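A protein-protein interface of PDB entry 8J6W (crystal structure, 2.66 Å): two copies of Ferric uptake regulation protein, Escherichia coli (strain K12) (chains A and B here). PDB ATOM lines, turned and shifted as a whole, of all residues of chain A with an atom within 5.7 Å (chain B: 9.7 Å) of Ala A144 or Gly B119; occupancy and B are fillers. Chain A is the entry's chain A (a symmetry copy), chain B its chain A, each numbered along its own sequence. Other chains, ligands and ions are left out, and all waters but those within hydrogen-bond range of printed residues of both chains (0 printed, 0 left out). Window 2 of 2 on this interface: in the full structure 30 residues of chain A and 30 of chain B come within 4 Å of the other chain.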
ATOM      1  N   HIS A 132     -29.118  27.517  21.074  1.00  0.00           N
ATOM      2  CA  HIS A 132     -28.234  28.367  21.855  1.00  0.00           C
ATOM      3  C   HIS A 132     -26.846  28.341  21.224  1.00  0.00           C
ATOM      4  O   HIS A 132     -26.493  27.402  20.498  1.00  0.00           O
ATOM      5  CB  HIS A 132     -28.184  27.907  23.331  1.00  0.00           C
ATOM      6  CG  HIS A 132     -29.511  27.983  24.015  1.00  0.00           C
ATOM      7  ND1 HIS A 132     -29.840  28.992  24.887  1.00  0.00           N
ATOM      8  CD2 HIS A 132     -30.612  27.200  23.911  1.00  0.00           C
ATOM      9  CE1 HIS A 132     -31.082  28.831  25.302  1.00  0.00           C
ATOM     10  NE2 HIS A 132     -31.574  27.751  24.721  1.00  0.00           N
ATOM     11  N   CYS A 133     -26.055  29.377  21.498  1.00  0.00           N
ATOM     12  CA  CYS A 133     -24.710  29.402  20.938  1.00  0.00           C
ATOM     13  C   CYS A 133     -23.894  28.267  21.531  1.00  0.00           C
ATOM     14  O   CYS A 133     -23.838  28.099  22.745  1.00  0.00           O
ATOM     15  CB  CYS A 133     -24.012  30.736  21.190  1.00  0.00           C
ATOM     16  SG  CYS A 133     -23.682  31.147  22.905  1.00  0.00           S
ATOM     17  N   ALA A 134     -23.254  27.497  20.662  1.00  0.00           N
ATOM     18  CA  ALA A 134     -22.545  26.311  21.101  1.00  0.00           C
ATOM     19  C   ALA A 134     -21.318  26.654  21.954  1.00  0.00           C
ATOM     20  O   ALA A 134     -21.052  25.974  22.952  1.00  0.00           O
ATOM     21  CB  ALA A 134     -22.171  25.478  19.882  1.00  0.00           C
ATOM     22  N   GLU A 135     -20.559  27.694  21.607  1.00  0.00           N
ATOM     23  CA  GLU A 135     -19.310  27.964  22.322  1.00  0.00           C
ATOM     24  C   GLU A 135     -19.154  29.440  22.644  1.00  0.00           C
ATOM     25  O   GLU A 135     -19.438  30.311  21.812  1.00  0.00           O
ATOM     26  CB  GLU A 135     -18.072  27.505  21.537  1.00  0.00           C
ATOM     27  CG  GLU A 135     -18.303  26.226  20.784  1.00  0.00           C
ATOM     28  CD  GLU A 135     -18.802  26.485  19.362  1.00  0.00           C
ATOM     29  OE1 GLU A 135     -19.079  27.672  19.011  1.00  0.00           O
ATOM     30  OE2 GLU A 135     -18.961  25.494  18.609  1.00  0.00           O
ATOM     31  N   CYS A 138     -22.036  34.364  21.965  1.00  0.00           N
ATOM     32  CA  CYS A 138     -22.235  35.047  20.693  1.00  0.00           C
ATOM     33  C   CYS A 138     -22.640  36.497  20.861  1.00  0.00           C
ATOM     34  O   CYS A 138     -22.599  37.245  19.884  1.00  0.00           O
ATOM     35  CB  CYS A 138     -23.307  34.334  19.882  1.00  0.00           C
ATOM     36  SG  CYS A 138     -24.783  34.048  20.859  1.00  0.00           S
ATOM     37  N   ASP A 141     -19.092  37.971  19.886  1.00  0.00           N
ATOM     38  CA  ASP A 141     -18.570  37.644  18.564  1.00  0.00           C
ATOM     39  C   ASP A 141     -19.648  37.811  17.501  1.00  0.00           C
ATOM     40  O   ASP A 141     -20.453  36.910  17.274  1.00  0.00           O
ATOM     41  CB  ASP A 141     -18.018  36.225  18.565  1.00  0.00           C
ATOM     42  CG  ASP A 141     -17.333  35.880  17.269  1.00  0.00           C
ATOM     43  OD1 ASP A 141     -17.023  36.828  16.509  1.00  0.00           O
ATOM     44  OD2 ASP A 141     -17.096  34.671  17.016  1.00  0.00           O
ATOM     45  N   GLU A 142     -19.616  38.943  16.792  1.00  0.00           N
ATOM     46  CA  GLU A 142     -20.581  39.165  15.677  1.00  0.00           C
ATOM     47  C   GLU A 142     -20.353  38.091  14.606  1.00  0.00           C
ATOM     48  O   GLU A 142     -21.294  37.827  13.832  1.00  0.00           O
ATOM     49  CB  GLU A 142     -20.441  40.585  15.124  1.00  0.00           C
ATOM     50  CG  GLU A 142     -19.169  40.816  14.326  1.00  0.00           C
ATOM     51  CD  GLU A 142     -18.075  41.587  15.046  1.00  0.00           C
ATOM     52  OE1 GLU A 142     -17.891  41.362  16.260  1.00  0.00           O
ATOM     53  OE2 GLU A 142     -17.407  42.408  14.389  1.00  0.00           O
ATOM     54  N   HIS A 143     -19.158  37.489  14.574  1.00  0.00           N
ATOM     55  CA  HIS A 143     -18.868  36.429  13.618  1.00  0.00           C
ATOM     56  C   HIS A 143     -19.374  35.052  14.067  1.00  0.00           C
ATOM     57  O   HIS A 143     -19.123  34.059  13.377  1.00  0.00           O
ATOM     58  CB  HIS A 143     -17.359  36.379  13.328  1.00  0.00           C
ATOM     59  CG  HIS A 143     -16.752  37.720  12.996  1.00  0.00           C
ATOM     60  ND1 HIS A 143     -15.954  38.426  13.872  1.00  0.00           N
ATOM     61  CD2 HIS A 143     -16.833  38.477  11.876  1.00  0.00           C
ATOM     62  CE1 HIS A 143     -15.572  39.558  13.308  1.00  0.00           C
ATOM     63  NE2 HIS A 143     -16.098  39.614  12.099  1.00  0.00           N
ATOM     64  N   ALA A 144     -20.123  34.978  15.175  1.00  0.00           N
ATOM     65  CA  ALA A 144     -20.441  33.679  15.777  1.00  0.00           C
ATOM     66  C   ALA A 144     -21.294  32.805  14.869  1.00  0.00           C
ATOM     67  O   ALA A 144     -21.133  31.584  14.872  1.00  0.00           O
ATOM     68  CB  ALA A 144     -21.148  33.865  17.120  1.00  0.00           C
ATOM     69  N   HIS A 145     -22.181  33.395  14.078  1.00  0.00           N
ATOM     70  CA  HIS A 145     -23.160  32.623  13.328  1.00  0.00           C
ATOM     71  C   HIS A 145     -22.970  32.709  11.813  1.00  0.00           C
ATOM     72  O   HIS A 145     -23.916  32.429  11.070  1.00  0.00           O
ATOM     73  CB  HIS A 145     -24.581  33.060  13.701  1.00  0.00           C
ATOM     74  CG  HIS A 145     -24.878  32.982  15.165  1.00  0.00           C
ATOM     75  ND1 HIS A 145     -24.565  31.877  15.929  1.00  0.00           N
ATOM     76  CD2 HIS A 145     -25.484  33.858  16.003  1.00  0.00           C
ATOM     77  CE1 HIS A 145     -24.945  32.085  17.180  1.00  0.00           C
ATOM     78  NE2 HIS A 145     -25.505  33.280  17.252  1.00  0.00           N
ATOM     79  N   GLU A 146     -21.783  33.088  11.329  1.00  0.00           N
ATOM     80  CA  GLU A 146     -21.488  33.061   9.898  1.00  0.00           C
ATOM     81  C   GLU A 146     -20.675  31.809   9.590  1.00  0.00           C
ATOM     82  O   GLU A 146     -19.588  31.623  10.151  1.00  0.00           O
ATOM     83  CB  GLU A 146     -20.702  34.293   9.449  1.00  0.00           C
ATOM     84  CG  GLU A 146     -20.879  35.584  10.239  1.00  0.00           C
ATOM     85  CD  GLU A 146     -19.719  36.569  10.003  1.00  0.00           C
ATOM     86  OE1 GLU A 146     -18.635  36.125   9.577  1.00  0.00           O
ATOM     87  OE2 GLU A 146     -19.883  37.783  10.249  1.00  0.00           O
ATOM     88  N   ARG B 112     -30.010  19.401  13.173  1.00  0.00           N
ATOM     89  CA  ARG B 112     -28.892  19.605  14.089  1.00  0.00           C
ATOM     90  C   ARG B 112     -27.635  20.011  13.331  1.00  0.00           C
ATOM     91  O   ARG B 112     -26.851  20.840  13.808  1.00  0.00           O
ATOM     92  CB  ARG B 112     -28.652  18.336  14.920  1.00  0.00           C
ATOM     93  CG  ARG B 112     -29.366  18.349  16.251  1.00  0.00           C
ATOM     94  CD  ARG B 112     -29.355  17.003  16.935  1.00  0.00           C
ATOM     95  NE  ARG B 112     -29.675  15.912  16.026  1.00  0.00           N
ATOM     96  CZ  ARG B 112     -30.548  14.957  16.312  1.00  0.00           C
ATOM     97  NH1 ARG B 112     -31.255  14.992  17.422  1.00  0.00           N
ATOM     98  NH2 ARG B 112     -30.728  13.953  15.455  1.00  0.00           N
ATOM     99  N   GLU B 113     -27.439  19.450  12.138  1.00  0.00           N
ATOM    100  CA  GLU B 113     -26.246  19.758  11.361  1.00  0.00           C
ATOM    101  C   GLU B 113     -26.277  21.209  10.865  1.00  0.00           C
ATOM    102  O   GLU B 113     -25.243  21.890  10.842  1.00  0.00           O
ATOM    103  CB  GLU B 113     -26.127  18.750  10.202  1.00  0.00           C
ATOM    104  CG  GLU B 113     -24.765  18.692   9.436  1.00  0.00           C
ATOM    105  CD  GLU B 113     -24.890  18.537   7.890  1.00  0.00           C
ATOM    106  OE1 GLU B 113     -25.088  19.557   7.175  1.00  0.00           O
ATOM    107  OE2 GLU B 113     -24.726  17.390   7.395  1.00  0.00           O
ATOM    108  N   ILE B 114     -27.460  21.712  10.488  1.00  0.00           N
ATOM    109  CA  ILE B 114     -27.551  23.075   9.962  1.00  0.00           C
ATOM    110  C   ILE B 114     -27.356  24.099  11.076  1.00  0.00           C
ATOM    111  O   ILE B 114     -26.743  25.152  10.869  1.00  0.00           O
ATOM    112  CB  ILE B 114     -28.890  23.276   9.229  1.00  0.00           C
ATOM    113  CG1 ILE B 114     -28.845  22.585   7.870  1.00  0.00           C
ATOM    114  CG2 ILE B 114     -29.234  24.774   9.079  1.00  0.00           C
ATOM    115  CD1 ILE B 114     -30.206  22.336   7.271  1.00  0.00           C
ATOM    116  N   ALA B 115     -27.888  23.826  12.269  1.00  0.00           N
ATOM    117  CA  ALA B 115     -27.654  24.746  13.378  1.00  0.00           C
ATOM    118  C   ALA B 115     -26.202  24.709  13.825  1.00  0.00           C
ATOM    119  O   ALA B 115     -25.641  25.739  14.218  1.00  0.00           O
ATOM    120  CB  ALA B 115     -28.570  24.417  14.555  1.00  0.00           C
ATOM    121  N   ALA B 116     -25.577  23.535  13.783  1.00  0.00           N
ATOM    122  CA  ALA B 116     -24.200  23.464  14.236  1.00  0.00           C
ATOM    123  C   ALA B 116     -23.265  24.143  13.252  1.00  0.00           C
ATOM    124  O   ALA B 116     -22.199  24.610  13.653  1.00  0.00           O
ATOM    125  CB  ALA B 116     -23.791  22.006  14.479  1.00  0.00           C
ATOM    126  N   LYS B 117     -23.646  24.226  11.978  1.00  0.00           N
ATOM    127  CA  LYS B 117     -22.803  24.932  11.025  1.00  0.00           C
ATOM    128  C   LYS B 117     -22.714  26.420  11.351  1.00  0.00           C
ATOM    129  O   LYS B 117     -21.694  27.048  11.062  1.00  0.00           O
ATOM    130  CB  LYS B 117     -23.320  24.755   9.594  1.00  0.00           C
ATOM    131  CG  LYS B 117     -22.806  23.519   8.840  1.00  0.00           C
ATOM    132  CD  LYS B 117     -23.557  23.347   7.497  1.00  0.00           C
ATOM    133  CE  LYS B 117     -22.852  22.382   6.525  1.00  0.00           C
ATOM    134  NZ  LYS B 117     -22.716  20.990   7.056  1.00  0.00           N
ATOM    135  N   HIS B 118     -23.759  27.001  11.943  1.00  0.00           N
ATOM    136  CA  HIS B 118     -23.799  28.430  12.223  1.00  0.00           C
ATOM    137  C   HIS B 118     -23.544  28.749  13.685  1.00  0.00           C
ATOM    138  O   HIS B 118     -24.022  29.778  14.171  1.00  0.00           O
ATOM    139  CB  HIS B 118     -25.142  29.021  11.804  1.00  0.00           C
ATOM    140  CG  HIS B 118     -25.386  29.001  10.327  1.00  0.00           C
ATOM    141  ND1 HIS B 118     -25.781  27.867   9.651  1.00  0.00           N
ATOM    142  CD2 HIS B 118     -25.330  29.983   9.405  1.00  0.00           C
ATOM    143  CE1 HIS B 118     -25.965  28.151   8.375  1.00  0.00           C
ATOM    144  NE2 HIS B 118     -25.682  29.426   8.198  1.00  0.00           N
ATOM    145  N   GLY B 119     -22.819  27.890  14.397  1.00  0.00           N
ATOM    146  CA  GLY B 119     -22.482  28.136  15.788  1.00  0.00           C
ATOM    147  C   GLY B 119     -23.560  27.837  16.809  1.00  0.00           C
ATOM    148  O   GLY B 119     -23.427  28.272  17.960  1.00  0.00           O
ATOM    149  N   ILE B 120     -24.616  27.113  16.443  1.00  0.00           N
ATOM    150  CA  ILE B 120     -25.795  26.951  17.285  1.00  0.00           C
ATOM    151  C   ILE B 120     -25.973  25.487  17.631  1.00  0.00           C
ATOM    152  O   ILE B 120     -25.799  24.623  16.769  1.00  0.00           O
ATOM    153  CB  ILE B 120     -27.073  27.501  16.610  1.00  0.00           C
ATOM    154  CG1 ILE B 120     -27.090  29.026  16.662  1.00  0.00           C
ATOM    155  CG2 ILE B 120     -28.343  26.907  17.229  1.00  0.00           C
ATOM    156  CD1 ILE B 120     -27.796  29.659  15.514  1.00  0.00           C
ATOM    157  N   ARG B 121     -26.305  25.219  18.903  1.00  0.00           N
ATOM    158  CA  ARG B 121     -26.739  23.901  19.364  1.00  0.00           C
ATOM    159  C   ARG B 121     -28.264  23.887  19.332  1.00  0.00           C
ATOM    160  O   ARG B 121     -28.912  24.617  20.089  1.00  0.00           O
ATOM    161  CB  ARG B 121     -26.211  23.604  20.772  1.00  0.00           C
ATOM    162  CG  ARG B 121     -26.773  22.324  21.392  1.00  0.00           C
ATOM    163  CD  ARG B 121     -26.337  22.013  22.854  1.00  0.00           C
ATOM    164  NE  ARG B 121     -26.240  23.171  23.735  1.00  0.00           N
ATOM    165  CZ  ARG B 121     -27.062  23.416  24.748  1.00  0.00           C
ATOM    166  NH1 ARG B 121     -28.083  22.624  25.016  1.00  0.00           N
ATOM    167  NH2 ARG B 121     -26.856  24.491  25.504  1.00  0.00           N
ATOM    168  N   LEU B 122     -28.837  23.068  18.456  1.00  0.00           N
ATOM    169  CA  LEU B 122     -30.288  23.025  18.308  1.00  0.00           C
ATOM    170  C   LEU B 122     -30.959  22.575  19.592  1.00  0.00           C
ATOM    171  O   LEU B 122     -30.699  21.464  20.071  1.00  0.00           O
ATOM    172  CB  LEU B 122     -30.665  22.073  17.177  1.00  0.00           C
ATOM    173  CG  LEU B 122     -32.137  22.117  16.792  1.00  0.00           C
ATOM    174  CD1 LEU B 122     -32.464  23.460  16.077  1.00  0.00           C
ATOM    175  CD2 LEU B 122     -32.399  20.960  15.891  1.00  0.00           C
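The backbone carbonyl oxygen of Ala B115 is in hydrogen-bond range of the backbone NH of Ile B120, at 2.8 Å.
ND1 of His B118 lies within hydrogen-bond range of O of Ile B114 (3.1 Å).
The side-chain sulfur (SG) of Cys A133 lies within hydrogen-bond range of the backbone NH (N) of Cys A138 (3.7 Å).
Printed residues of chain B within 4 Å of His A132: Ile B120 and Arg B121.
Printed residues of chain B within 4 Å of Cys A133: Gly B119 (3.4 Å).
Asp A141 touches none of the printed residues of chain B.
Ala A144 touches just these residues of chain B: His B118 (3.5 Å) and Gly B119 (3.8 Å).
Of the printed residues of chain B, His A145 touches His B118 and Ile B120.
Ile B114 touches none of the printed residues of chain A.
Printed residues of chain A within 4 Å of His B118: Ala A144 (3.5 Å) and His A145 (2.8 Å).
The nearest residue of chain B that does not touch Ala A144 is Ile B120 (5.9 Å).
The backbone carbonyl oxygen (O) of Gly B119 is in hydrogen-bond range of the backbone NH (N) of Ala A134 (2.8 Å).
O of His B118 sits at hydrogen-bond distance from ND1 of His A145, 2.8 Å away.
N of Arg B121 lies within hydrogen-bond range of O of His A132 (2.7 Å).
The backbone carbonyl oxygen of Ala A144 sits close to the backbone carbonyl oxygen of His B118.
Ile B120 touches His A132 (CA to O, 3.3 Å).
Gly B119 touches Cys A133.
Gly B119 touches Ala A144.
Ile B120 touches His A145.
Hydrophobic or aromatic side chains of chain B within 4 Å of the printed part of chain A: His B118 and Ile B120.
Printed residues of chain A that touch a printed residue of chain B: His A132, Cys A133, Ala A134, Ala A144 and His A145.
Hydrophobic or aromatic side chains of chain A that line the printed part of chain B: Ala A134 and His A145.
Among the printed residues, 8 pairs touch across the chains.
Among the printed residues, no Asp or Glu carboxylate lies within 4 Å of a Lys or Arg side-chain nitrogen of the other chain.
No position is printed for both chains.
Of the 8 pairs that touch across the chains among the printed residues, none has its exchanged pair printed and touching as well.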
